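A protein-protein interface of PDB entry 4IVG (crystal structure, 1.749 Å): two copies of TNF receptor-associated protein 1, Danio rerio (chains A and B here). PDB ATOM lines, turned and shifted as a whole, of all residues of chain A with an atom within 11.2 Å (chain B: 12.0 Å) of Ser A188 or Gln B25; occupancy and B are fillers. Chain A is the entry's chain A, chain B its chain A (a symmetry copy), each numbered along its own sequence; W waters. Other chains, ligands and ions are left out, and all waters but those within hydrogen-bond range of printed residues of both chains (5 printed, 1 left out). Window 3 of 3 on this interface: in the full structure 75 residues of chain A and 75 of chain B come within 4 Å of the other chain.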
ATOM      1  N   GLN A 100      10.818  10.031  15.356  1.00  0.00           N
ATOM      2  CA  GLN A 100      11.136   9.205  16.525  1.00  0.00           C
ATOM      3  C   GLN A 100      10.372   9.741  17.728  1.00  0.00           C
ATOM      4  O   GLN A 100      10.349  10.951  17.963  1.00  0.00           O
ATOM      5  CB  GLN A 100      12.647   9.218  16.802  1.00  0.00           C
ATOM      6  CG  GLN A 100      13.072   8.320  17.971  1.00  0.00           C
ATOM      7  CD  GLN A 100      14.569   8.292  18.179  1.00  0.00           C
ATOM      8  OE1 GLN A 100      15.335   8.580  17.261  1.00  0.00           O
ATOM      9  NE2 GLN A 100      14.997   7.943  19.393  1.00  0.00           N
ATOM     10  N   LYS A 108       8.340  -7.705  19.670  1.00  0.00           N
ATOM     11  CA  LYS A 108       8.196  -8.383  18.384  1.00  0.00           C
ATOM     12  C   LYS A 108       6.745  -8.726  18.051  1.00  0.00           C
ATOM     13  O   LYS A 108       6.294  -8.517  16.922  1.00  0.00           O
ATOM     14  CB  LYS A 108       9.056  -9.640  18.304  1.00  0.00           C
ATOM     15  CG  LYS A 108       8.946 -10.288  16.944  1.00  0.00           C
ATOM     16  CD  LYS A 108       9.921 -11.420  16.757  1.00  0.00           C
ATOM     17  CE  LYS A 108       9.575 -12.170  15.481  1.00  0.00           C
ATOM     18  NZ  LYS A 108      10.720 -12.984  14.986  1.00  0.00           N
ATOM     19  N   VAL A 160      11.355   0.571  10.631  1.00  0.00           N
ATOM     20  CA  VAL A 160      10.910   0.916  11.971  1.00  0.00           C
ATOM     21  C   VAL A 160      11.847   0.253  12.972  1.00  0.00           C
ATOM     22  O   VAL A 160      12.049  -0.972  12.935  1.00  0.00           O
ATOM     23  CB  VAL A 160       9.475   0.410  12.222  1.00  0.00           C
ATOM     24  CG1 VAL A 160       9.035   0.714  13.664  1.00  0.00           C
ATOM     25  CG2 VAL A 160       8.472   1.005  11.206  1.00  0.00           C
ATOM     26  N   TYR A 161      12.438   1.059  13.851  1.00  0.00           N
ATOM     27  CA  TYR A 161      13.244   0.519  14.952  1.00  0.00           C
ATOM     28  C   TYR A 161      12.470   0.780  16.227  1.00  0.00           C
ATOM     29  O   TYR A 161      12.088   1.922  16.489  1.00  0.00           O
ATOM     30  CB  TYR A 161      14.582   1.240  15.038  1.00  0.00           C
ATOM     31  CG  TYR A 161      15.374   1.210  13.758  1.00  0.00           C
ATOM     32  CD1 TYR A 161      15.166   2.165  12.766  1.00  0.00           C
ATOM     33  CD2 TYR A 161      16.322   0.216  13.526  1.00  0.00           C
ATOM     34  CE1 TYR A 161      15.882   2.140  11.581  1.00  0.00           C
ATOM     35  CE2 TYR A 161      17.052   0.186  12.340  1.00  0.00           C
ATOM     36  CZ  TYR A 161      16.823   1.148  11.377  1.00  0.00           C
ATOM     37  OH  TYR A 161      17.543   1.133  10.198  1.00  0.00           O
ATOM     38  N   SER A 162      12.248  -0.263  17.017  1.00  0.00           N
ATOM     39  CA  SER A 162      11.460  -0.105  18.232  1.00  0.00           C
ATOM     40  C   SER A 162      12.013  -0.899  19.402  1.00  0.00           C
ATOM     41  O   SER A 162      12.501  -2.028  19.258  1.00  0.00           O
ATOM     42  CB  SER A 162       9.999  -0.481  17.980  1.00  0.00           C
ATOM     43  OG  SER A 162       9.158   0.122  18.946  1.00  0.00           O
ATOM     44  N   GLN A 163      11.932  -0.281  20.571  1.00  0.00           N
ATOM     45  CA  GLN A 163      12.371  -0.910  21.803  1.00  0.00           C
ATOM     46  C   GLN A 163      11.270  -0.714  22.835  1.00  0.00           C
ATOM     47  O   GLN A 163      10.894   0.423  23.133  1.00  0.00           O
ATOM     48  CB  GLN A 163      13.668  -0.264  22.287  1.00  0.00           C
ATOM     49  CG  GLN A 163      14.034  -0.664  23.701  1.00  0.00           C
ATOM     50  CD  GLN A 163      14.529  -2.094  23.789  1.00  0.00           C
ATOM     51  OE1 GLN A 163      15.604  -2.430  23.272  1.00  0.00           O
ATOM     52  NE2 GLN A 163      13.748  -2.949  24.440  1.00  0.00           N
ATOM     53  N   ASP A 168      13.316  -6.898  30.077  1.00  0.00           N
ATOM     54  CA  ASP A 168      14.631  -6.956  29.445  1.00  0.00           C
ATOM     55  C   ASP A 168      14.366  -7.263  27.949  1.00  0.00           C
ATOM     56  O   ASP A 168      15.197  -7.921  27.295  1.00  0.00           O
ATOM     57  CB  ASP A 168      15.671  -7.966  30.028  1.00  0.00           C
ATOM     58  CG  ASP A 168      15.988  -7.728  31.552  1.00  0.00           C
ATOM     59  OD1 ASP A 168      15.934  -6.586  32.040  1.00  0.00           O
ATOM     60  OD2 ASP A 168      16.296  -8.689  32.276  1.00  0.00           O
ATOM     61  N   ALA A 169      13.249  -6.773  27.404  1.00  0.00           N
ATOM     62  CA  ALA A 169      12.898  -7.015  25.993  1.00  0.00           C
ATOM     63  C   ALA A 169      13.955  -6.463  25.024  1.00  0.00           C
ATOM     64  O   ALA A 169      14.500  -5.385  25.255  1.00  0.00           O
ATOM     65  CB  ALA A 169      11.531  -6.412  25.671  1.00  0.00           C
ATOM     66  N   PRO A 170      14.247  -7.198  23.931  1.00  0.00           N
ATOM     67  CA  PRO A 170      15.268  -6.753  22.965  1.00  0.00           C
ATOM     68  C   PRO A 170      14.738  -5.696  21.997  1.00  0.00           C
ATOM     69  O   PRO A 170      13.526  -5.456  21.963  1.00  0.00           O
ATOM     70  CB  PRO A 170      15.608  -8.038  22.207  1.00  0.00           C
ATOM     71  CG  PRO A 170      14.358  -8.829  22.260  1.00  0.00           C
ATOM     72  CD  PRO A 170      13.698  -8.521  23.581  1.00  0.00           C
ATOM     73  N   GLY A 171      15.626  -5.066  21.229  1.00  0.00           N
ATOM     74  CA  GLY A 171      15.211  -4.086  20.233  1.00  0.00           C
ATOM     75  C   GLY A 171      14.942  -4.771  18.903  1.00  0.00           C
ATOM     76  O   GLY A 171      15.452  -5.871  18.657  1.00  0.00           O
ATOM     77  N   TYR A 172      14.147  -4.135  18.045  1.00  0.00           N
ATOM     78  CA  TYR A 172      13.789  -4.730  16.759  1.00  0.00           C
ATOM     79  C   TYR A 172      13.827  -3.766  15.592  1.00  0.00           C
ATOM     80  O   TYR A 172      13.589  -2.568  15.742  1.00  0.00           O
ATOM     81  CB  TYR A 172      12.399  -5.365  16.828  1.00  0.00           C
ATOM     82  CG  TYR A 172      12.351  -6.607  17.678  1.00  0.00           C
ATOM     83  CD1 TYR A 172      12.710  -7.840  17.153  1.00  0.00           C
ATOM     84  CD2 TYR A 172      11.959  -6.545  19.005  1.00  0.00           C
ATOM     85  CE1 TYR A 172      12.684  -8.990  17.934  1.00  0.00           C
ATOM     86  CE2 TYR A 172      11.921  -7.689  19.799  1.00  0.00           C
ATOM     87  CZ  TYR A 172      12.285  -8.906  19.256  1.00  0.00           C
ATOM     88  OH  TYR A 172      12.251 -10.038  20.036  1.00  0.00           O
ATOM     89  N   LYS A 173      14.132  -4.324  14.423  1.00  0.00           N
ATOM     90  CA  LYS A 173      13.949  -3.629  13.151  1.00  0.00           C
ATOM     91  C   LYS A 173      12.883  -4.324  12.311  1.00  0.00           C
ATOM     92  O   LYS A 173      12.946  -5.527  12.062  1.00  0.00           O
ATOM     93  CB  LYS A 173      15.268  -3.540  12.360  1.00  0.00           C
ATOM     94  CG  LYS A 173      15.099  -2.721  11.069  1.00  0.00           C
ATOM     95  CD  LYS A 173      16.406  -2.663  10.283  1.00  0.00           C
ATOM     96  CE  LYS A 173      16.243  -1.850   8.994  1.00  0.00           C
ATOM     97  NZ  LYS A 173      17.569  -1.789   8.275  1.00  0.00           N
ATOM     98  N   TRP A 174      11.906  -3.539  11.884  1.00  0.00           N
ATOM     99  CA  TRP A 174      10.801  -3.968  11.022  1.00  0.00           C
ATOM    100  C   TRP A 174      11.032  -3.229   9.715  1.00  0.00           C
ATOM    101  O   TRP A 174      11.362  -2.040   9.734  1.00  0.00           O
ATOM    102  CB  TRP A 174       9.483  -3.520  11.660  1.00  0.00           C
ATOM    103  CG  TRP A 174       8.183  -3.856  10.931  1.00  0.00           C
ATOM    104  CD1 TRP A 174       7.287  -4.846  11.268  1.00  0.00           C
ATOM    105  CD2 TRP A 174       7.611  -3.175   9.797  1.00  0.00           C
ATOM    106  NE1 TRP A 174       6.210  -4.823  10.415  1.00  0.00           N
ATOM    107  CE2 TRP A 174       6.381  -3.818   9.502  1.00  0.00           C
ATOM    108  CE3 TRP A 174       8.013  -2.087   9.006  1.00  0.00           C
ATOM    109  CZ2 TRP A 174       5.554  -3.414   8.445  1.00  0.00           C
ATOM    110  CZ3 TRP A 174       7.191  -1.687   7.953  1.00  0.00           C
ATOM    111  CH2 TRP A 174       5.972  -2.351   7.685  1.00  0.00           C
ATOM    112  N   GLU A 183       9.702  -7.668   6.962  1.00  0.00           N
ATOM    113  CA  GLU A 183      10.685  -8.465   7.682  1.00  0.00           C
ATOM    114  C   GLU A 183      10.923  -7.879   9.052  1.00  0.00           C
ATOM    115  O   GLU A 183      10.827  -6.657   9.241  1.00  0.00           O
ATOM    116  CB  GLU A 183      12.026  -8.455   6.950  1.00  0.00           C
ATOM    117  CG  GLU A 183      12.018  -8.949   5.532  1.00  0.00           C
ATOM    118  CD  GLU A 183      13.431  -9.109   5.003  1.00  0.00           C
ATOM    119  OE1 GLU A 183      14.331  -8.399   5.504  1.00  0.00           O
ATOM    120  OE2 GLU A 183      13.648  -9.958   4.111  1.00  0.00           O
ATOM    121  N   VAL A 184      11.267  -8.746   9.997  1.00  0.00           N
ATOM    122  CA  VAL A 184      11.595  -8.329  11.351  1.00  0.00           C
ATOM    123  C   VAL A 184      12.855  -9.052  11.810  1.00  0.00           C
ATOM    124  O   VAL A 184      12.993 -10.266  11.615  1.00  0.00           O
ATOM    125  CB  VAL A 184      10.448  -8.628  12.337  1.00  0.00           C
ATOM    126  CG1 VAL A 184      10.799  -8.124  13.734  1.00  0.00           C
ATOM    127  CG2 VAL A 184       9.130  -7.999  11.851  1.00  0.00           C
ATOM    128  N   ALA A 185      13.771  -8.295  12.407  1.00  0.00           N
ATOM    129  CA  ALA A 185      14.974  -8.850  13.016  1.00  0.00           C
ATOM    130  C   ALA A 185      15.292  -8.121  14.317  1.00  0.00           C
ATOM    131  O   ALA A 185      14.940  -6.946  14.480  1.00  0.00           O
ATOM    132  CB  ALA A 185      16.145  -8.762  12.051  1.00  0.00           C
ATOM    133  N   GLU A 186      15.935  -8.824  15.245  1.00  0.00           N
ATOM    134  CA  GLU A 186      16.491  -8.193  16.437  1.00  0.00           C
ATOM    135  C   GLU A 186      17.520  -7.140  16.030  1.00  0.00           C
ATOM    136  O   GLU A 186      18.233  -7.310  15.036  1.00  0.00           O
ATOM    137  CB  GLU A 186      17.152  -9.231  17.341  1.00  0.00           C
ATOM    138  CG  GLU A 186      16.185 -10.231  17.914  1.00  0.00           C
ATOM    139  CD  GLU A 186      16.784 -10.990  19.080  1.00  0.00           C
ATOM    140  OE1 GLU A 186      17.999 -10.825  19.335  1.00  0.00           O
ATOM    141  OE2 GLU A 186      16.038 -11.744  19.741  1.00  0.00           O
ATOM    142  N   ALA A 187      17.584  -6.054  16.797  1.00  0.00           N
ATOM    143  CA  ALA A 187      18.476  -4.929  16.512  1.00  0.00           C
ATOM    144  C   ALA A 187      19.098  -4.382  17.798  1.00  0.00           C
ATOM    145  O   ALA A 187      18.446  -4.329  18.845  1.00  0.00           O
ATOM    146  CB  ALA A 187      17.723  -3.820  15.763  1.00  0.00           C
ATOM    147  N   SER A 188      20.360  -3.966  17.719  1.00  0.00           N
ATOM    148  CA  SER A 188      21.049  -3.364  18.858  1.00  0.00           C
ATOM    149  C   SER A 188      21.001  -1.842  18.734  1.00  0.00           C
ATOM    150  O   SER A 188      20.751  -1.314  17.648  1.00  0.00           O
ATOM    151  CB  SER A 188      22.510  -3.825  18.899  1.00  0.00           C
ATOM    152  OG  SER A 188      23.206  -3.355  17.761  1.00  0.00           O
ATOM    153  N   GLY A 189      21.256  -1.137  19.833  1.00  0.00           N
ATOM    154  CA  GLY A 189      21.296   0.314  19.815  1.00  0.00           C
ATOM    155  C   GLY A 189      19.967   1.022  19.554  1.00  0.00           C
ATOM    156  O   GLY A 189      19.974   2.166  19.091  1.00  0.00           O
ATOM    157  N   VAL A 190      18.836   0.361  19.834  1.00  0.00           N
ATOM    158  CA  VAL A 190      17.534   1.021  19.662  1.00  0.00           C
ATOM    159  C   VAL A 190      17.134   1.656  20.975  1.00  0.00           C
ATOM    160  O   VAL A 190      17.058   0.987  22.009  1.00  0.00           O
ATOM    161  CB  VAL A 190      16.393   0.056  19.244  1.00  0.00           C
ATOM    162  CG1 VAL A 190      15.076   0.859  18.970  1.00  0.00           C
ATOM    163  CG2 VAL A 190      16.792  -0.789  18.037  1.00  0.00           C
ATOM    164  N   ARG A 191      16.854   2.948  20.940  1.00  0.00           N
ATOM    165  CA  ARG A 191      16.436   3.638  22.141  1.00  0.00           C
ATOM    166  C   ARG A 191      14.968   3.363  22.428  1.00  0.00           C
ATOM    167  O   ARG A 191      14.169   3.217  21.498  1.00  0.00           O
ATOM    168  CB  ARG A 191      16.632   5.137  21.971  1.00  0.00           C
ATOM    169  CG  ARG A 191      16.043   5.940  23.102  1.00  0.00           C
ATOM    170  CD  ARG A 191      16.276   7.398  22.894  1.00  0.00           C
ATOM    171  NE  ARG A 191      15.635   8.202  23.924  1.00  0.00           N
ATOM    172  CZ  ARG A 191      16.066   9.402  24.286  1.00  0.00           C
ATOM    173  NH1 ARG A 191      17.147   9.910  23.704  1.00  0.00           N
ATOM    174  NH2 ARG A 191      15.429  10.086  25.228  1.00  0.00           N
ATOM    175  N   GLN A 192      14.628   3.307  23.715  1.00  0.00           N
ATOM    176  CA  GLN A 192      13.252   3.206  24.189  1.00  0.00           C
ATOM    177  C   GLN A 192      12.333   4.059  23.327  1.00  0.00           C
ATOM    178  O   GLN A 192      12.569   5.256  23.099  1.00  0.00           O
ATOM    179  CB  GLN A 192      13.172   3.669  25.649  1.00  0.00           C
ATOM    180  CG  GLN A 192      11.761   3.751  26.184  1.00  0.00           C
ATOM    181  CD  GLN A 192      11.074   2.418  26.109  1.00  0.00           C
ATOM    182  OE1 GLN A 192      11.690   1.386  26.374  1.00  0.00           O
ATOM    183  NE2 GLN A 192       9.799   2.422  25.720  1.00  0.00           N
ATOM    184  N   GLY A 193      11.298   3.428  22.786  1.00  0.00           N
ATOM    185  CA  GLY A 193      10.416   4.122  21.869  1.00  0.00           C
ATOM    186  C   GLY A 193      10.528   3.583  20.451  1.00  0.00           C
ATOM    187  O   GLY A 193      10.899   2.425  20.250  1.00  0.00           O
ATOM    188  N   LYS A 195      11.506   4.637  16.211  1.00  0.00           N
ATOM    189  CA  LYS A 195      11.984   5.518  15.142  1.00  0.00           C
ATOM    190  C   LYS A 195      11.556   4.963  13.783  1.00  0.00           C
ATOM    191  O   LYS A 195      11.772   3.784  13.487  1.00  0.00           O
ATOM    192  CB  LYS A 195      13.513   5.616  15.197  1.00  0.00           C
ATOM    193  CG  LYS A 195      14.079   6.462  14.062  1.00  0.00           C
ATOM    194  CD  LYS A 195      15.528   6.892  14.324  1.00  0.00           C
ATOM    195  CE  LYS A 195      16.503   5.779  14.019  1.00  0.00           C
ATOM    196  NZ  LYS A 195      17.913   6.220  14.255  1.00  0.00           N
ATOM    197  N   THR B  19      19.637   9.797  16.056  1.00  0.00           N
ATOM    198  CA  THR B  19      21.034   9.440  15.860  1.00  0.00           C
ATOM    199  C   THR B  19      21.116   8.036  15.260  1.00  0.00           C
ATOM    200  O   THR B  19      20.310   7.165  15.578  1.00  0.00           O
ATOM    201  CB  THR B  19      21.821   9.551  17.195  1.00  0.00           C
ATOM    202  OG1 THR B  19      23.188   9.162  17.001  1.00  0.00           O
ATOM    203  CG2 THR B  19      21.182   8.688  18.290  1.00  0.00           C
ATOM    204  N   ASP B  20      22.078   7.822  14.371  1.00  0.00           N
ATOM    205  CA  ASP B  20      22.193   6.552  13.673  1.00  0.00           C
ATOM    206  C   ASP B  20      22.949   5.549  14.552  1.00  0.00           C
ATOM    207  O   ASP B  20      24.171   5.442  14.473  1.00  0.00           O
ATOM    208  CB  ASP B  20      22.899   6.776  12.327  1.00  0.00           C
ATOM    209  CG  ASP B  20      23.419   5.488  11.698  1.00  0.00           C
ATOM    210  OD1 ASP B  20      22.655   4.493  11.656  1.00  0.00           O
ATOM    211  OD2 ASP B  20      24.591   5.463  11.255  1.00  0.00           O
ATOM    212  N   THR B  21      22.225   4.821  15.403  1.00  0.00           N
ATOM    213  CA  THR B  21      22.868   3.946  16.388  1.00  0.00           C
ATOM    214  C   THR B  21      22.590   2.462  16.162  1.00  0.00           C
ATOM    215  O   THR B  21      23.218   1.601  16.777  1.00  0.00           O
ATOM    216  CB  THR B  21      22.399   4.286  17.819  1.00  0.00           C
ATOM    217  OG1 THR B  21      20.966   4.312  17.844  1.00  0.00           O
ATOM    218  CG2 THR B  21      22.946   5.635  18.270  1.00  0.00           C
ATOM    219  N   GLU B  22      21.634   2.170  15.288  1.00  0.00           N
ATOM    220  CA  GLU B  22      21.075   0.828  15.182  1.00  0.00           C
ATOM    221  C   GLU B  22      21.809  -0.113  14.215  1.00  0.00           C
ATOM    222  O   GLU B  22      22.254   0.291  13.137  1.00  0.00           O
ATOM    223  CB  GLU B  22      19.585   0.933  14.824  1.00  0.00           C
ATOM    224  CG  GLU B  22      18.790   1.781  15.808  1.00  0.00           C
ATOM    225  CD  GLU B  22      18.695   3.263  15.412  1.00  0.00           C
ATOM    226  OE1 GLU B  22      19.387   3.700  14.450  1.00  0.00           O
ATOM    227  OE2 GLU B  22      17.928   3.988  16.083  1.00  0.00           O
ATOM    228  N   ASN B  23      21.962  -1.365  14.636  1.00  0.00           N
ATOM    229  CA  ASN B  23      22.429  -2.427  13.761  1.00  0.00           C
ATOM    230  C   ASN B  23      21.596  -3.679  13.982  1.00  0.00           C
ATOM    231  O   ASN B  23      21.168  -3.947  15.101  1.00  0.00           O
ATOM    232  CB  ASN B  23      23.895  -2.745  14.033  1.00  0.00           C
ATOM    233  CG  ASN B  23      24.827  -1.714  13.446  1.00  0.00           C
ATOM    234  OD1 ASN B  23      25.426  -0.928  14.174  1.00  0.00           O
ATOM    235  ND2 ASN B  23      24.963  -1.716  12.126  1.00  0.00           N
ATOM    236  N   VAL B  24      21.358  -4.427  12.908  1.00  0.00           N
ATOM    237  CA  VAL B  24      20.600  -5.672  12.977  1.00  0.00           C
ATOM    238  C   VAL B  24      21.484  -6.732  13.626  1.00  0.00           C
ATOM    239  O   VAL B  24      22.679  -6.819  13.320  1.00  0.00           O
ATOM    240  CB  VAL B  24      20.137  -6.131  11.577  1.00  0.00           C
ATOM    241  CG1 VAL B  24      19.563  -7.556  11.621  1.00  0.00           C
ATOM    242  CG2 VAL B  24      19.138  -5.157  10.991  1.00  0.00           C
ATOM    243  N   GLN B  25      20.879  -7.526  14.511  1.00  0.00           N
ATOM    244  CA  GLN B  25      21.560  -8.480  15.394  1.00  0.00           C
ATOM    245  C   GLN B  25      21.305  -9.938  15.045  1.00  0.00           C
ATOM    246  O   GLN B  25      22.069 -10.812  15.427  1.00  0.00           O
ATOM    247  CB  GLN B  25      21.008  -8.312  16.808  1.00  0.00           C
ATOM    248  CG  GLN B  25      21.861  -7.566  17.783  1.00  0.00           C
ATOM    249  CD  GLN B  25      21.277  -7.650  19.174  1.00  0.00           C
ATOM    250  OE1 GLN B  25      20.348  -8.428  19.423  1.00  0.00           O
ATOM    251  NE2 GLN B  25      21.811  -6.853  20.092  1.00  0.00           N
ATOM    252  N   GLY B  26      20.185 -10.215  14.397  1.00  0.00           N
ATOM    253  CA  GLY B  26      19.783 -11.591  14.170  1.00  0.00           C
ATOM    254  C   GLY B  26      19.315 -11.778  12.747  1.00  0.00           C
ATOM    255  O   GLY B  26      19.306 -10.824  11.959  1.00  0.00           O
ATOM    256  N   SER B  27      18.930 -13.000  12.405  1.00  0.00           N
ATOM    257  CA  SER B  27      18.382 -13.257  11.085  1.00  0.00           C
ATOM    258  C   SER B  27      17.023 -12.579  10.987  1.00  0.00           C
ATOM    259  O   SER B  27      16.353 -12.351  12.000  1.00  0.00           O
ATOM    260  CB  SER B  27      18.251 -14.759  10.826  1.00  0.00           C
ATOM    261  OG  SER B  27      17.346 -15.368  11.731  1.00  0.00           O
ATOM    262  N   PHE B  28      16.627 -12.246   9.765  1.00  0.00           N
ATOM    263  CA  PHE B  28      15.301 -11.693   9.532  1.00  0.00           C
ATOM    264  C   PHE B  28      14.271 -12.824   9.426  1.00  0.00           C
ATOM    265  O   PHE B  28      14.574 -13.913   8.927  1.00  0.00           O
ATOM    266  CB  PHE B  28      15.296 -10.824   8.267  1.00  0.00           C
ATOM    267  CG  PHE B  28      15.854  -9.431   8.473  1.00  0.00           C
ATOM    268  CD1 PHE B  28      15.018  -8.376   8.811  1.00  0.00           C
ATOM    269  CD2 PHE B  28      17.211  -9.175   8.317  1.00  0.00           C
ATOM    270  CE1 PHE B  28      15.526  -7.090   8.997  1.00  0.00           C
ATOM    271  CE2 PHE B  28      17.723  -7.893   8.502  1.00  0.00           C
ATOM    272  CZ  PHE B  28      16.875  -6.852   8.844  1.00  0.00           C
ATOM    273  N   SER B  29      13.074 -12.573   9.947  1.00  0.00           N
ATOM    274  CA  SER B  29      11.912 -13.419   9.702  1.00  0.00           C
ATOM    275  C   SER B  29      11.032 -12.718   8.666  1.00  0.00           C
ATOM    276  O   SER B  29      10.858 -11.499   8.720  1.00  0.00           O
ATOM    277  CB  SER B  29      11.129 -13.655  11.003  1.00  0.00           C
ATOM    278  OG  SER B  29      10.831 -12.442  11.672  1.00  0.00           O
HETATM  279  O   HOH W   1      16.577   4.332  18.335  1.00  0.00           O
HETATM  280  O   HOH W   2      24.372  -1.160  17.046  1.00  0.00           O
HETATM  281  O   HOH W   3      20.885   1.314  10.995  1.00  0.00           O
HETATM  282  O   HOH W   4      17.695   7.600  16.821  1.00  0.00           O
HETATM  283  O   HOH W   5      16.440 -11.722  14.438  1.00  0.00           O
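The backbone NH of Ala A187 sits at hydrogen-bond distance from the backbone carbonyl oxygen of Gly A171 (2.8 Å).
N of Lys A173 lies within hydrogen-bond range of O of Ala A185 (2.7 Å).
The backbone carbonyl oxygen of Tyr A161 sits at hydrogen-bond distance from the backbone NH of Lys A195.
OH of Tyr A161 lies close to NZ of Lys A173 (3.5 Å).
No position is printed for both chains.
The side-chain amino group (NZ) of Lys A108 is in hydrogen-bond range of the side-chain hydroxyl (OG) of Ser B29.
The side-chain hydroxyl of Thr B21 sits at hydrogen-bond distance from the backbone carbonyl oxygen of Gly A189, 2.7 Å away.
The backbone carbonyl oxygen (O) of Glu A186 is in hydrogen-bond range of the backbone NH (N) of Gln B25.
O of Val A184 sits at hydrogen-bond distance from N of Ser B29 (2.8 Å).
O of Thr B19 sits at hydrogen-bond distance from NZ of Lys A195 (2.9 Å).
The side-chain amino group (NZ) of Lys A195 lies within salt-bridge range of the side-chain carboxylate (OE2) of Glu B22, at 2.9 Å.
The backbone NH (N) of Ser A188 sits at hydrogen-bond distance from the backbone carbonyl oxygen (O) of Asn B23 (2.7 Å).
Ser A188 touches just these residues of chain B: Thr B21 (3.9 Å), Glu B22 (3.3 Å), Asn B23 (2.7 Å) and Gln B25 (3.3 Å).
No residue of chain B comes within 4 Å of Pro A170.
No residue of chain B comes within 4 Å of Gly A171.
Ala A185 touches just these residues of chain B: Val B24, Gly B26, Ser B27 and Phe B28.
Glu A186 touches just these residues of chain B: Val B24, Gln B25 and Gly B26.
Of chain B, only Asn B23 (3.2 Å) comes within 4 Å of Ala A187.
Of chain B, only Thr B21 and Glu B22 come within 4 Å of Gly A189.
Glu B22 touches just these residues of chain A: Tyr A161 (3.6 Å), Ser A188 (3.3 Å), Gly A189 (3.5 Å), Val A190 (3.9 Å) and Lys A195 (2.9 Å).
Asn B23 touches just these residues of chain A: Ala A187 (3.2 Å) and Ser A188 (2.7 Å).
Of chain A, only Lys A173, Ala A185 and Glu A186 come within 4 Å of Val B24.
Gly B26 touches two residues of chain A.
Of the printed residues of chain A, Ser B29 touches Lys A108, Glu A183 and Val A184.
Of the printed residues of chain B, Lys A108 touches Ser B29 (3.4 Å).
Of the printed residues of chain A, Phe B28 touches Glu A183 (3.4 Å), Val A184 (3.4 Å) and Ala A185 (3.5 Å).
Ser A162 touches none of the printed residues of chain B.
The nearest printed residue of chain A that does not touch Phe B28 is Lys A173 (4.3 Å).
Water W5 lies within hydrogen-bond range of the backbone carbonyl oxygen (O) of Ser B27 (2.5 Å) and the backbone NH (N) of Glu A186 (3.1 Å).
Water W2 lies within hydrogen-bond range of OG of Ser A188 (2.6 Å), O of Thr B21 (3.0 Å) and OD1 of Asn B23 (3.1 Å).
Water W4 lies within hydrogen-bond range of OE1 of Gln A100 (2.6 Å), NZ of Lys A195 (2.9 Å) and O of Thr B19 (2.9 Å).
Water W1 lies within hydrogen-bond range of the side-chain carboxylate (OE2) of Glu B22 (2.6 Å) and the backbone NH (N) of Arg A191 (3.0 Å).
Water W3 lies within hydrogen-bond range of O of Glu B22 (2.7 Å) and OH of Tyr A161 (3.4 Å).
Of the 25 printed residues of chain A, 12 touch a printed residue of chain B.
Hydrophobic or aromatic side chains of chain A that line the printed part of chain B: Tyr A161, Val A184, Ala A185, Ala A187 and Val A190.
Of the 11 printed residues of chain B, 10 touch a printed residue of chain A.
Printed residues of chain B that touch a printed residue of chain A: Thr B19, Thr B21, Glu B22, Asn B23, Val B24, Gln B25, Gly B26, Ser B27, Phe B28 and Ser B29.
Hydrophobic or aromatic side chains of chain B that line the printed part of chain A: Val B24 and Phe B28.
Among the printed residues, Asp or Glu carboxylates within 4 Å of a Lys or Arg side-chain nitrogen of the other chain: Lys A195 with Glu B22 (2.9 Å).
Among the printed residues, pairs that only touch across the chains: Ala A187 with Asn B23, Glu A183 with Ser B29, Ser A188 with Glu B22, Ser A188 with Gln B25, Glu A183 with Phe B28, Val A184 with Phe B28, Ala A185 with Phe B28, Gly A189 with Glu B22, Glu A186 with Val B24, Glu A186 with Gly B26, Tyr A161 with Glu B22, Ala A185 with Ser B27, Ala A185 with Val B24, Lys A173 with Val B24, Ala A185 with Gly B26, Ser A188 with Thr B21, Val A190 with Glu B22 and Val A184 with Ser B27.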
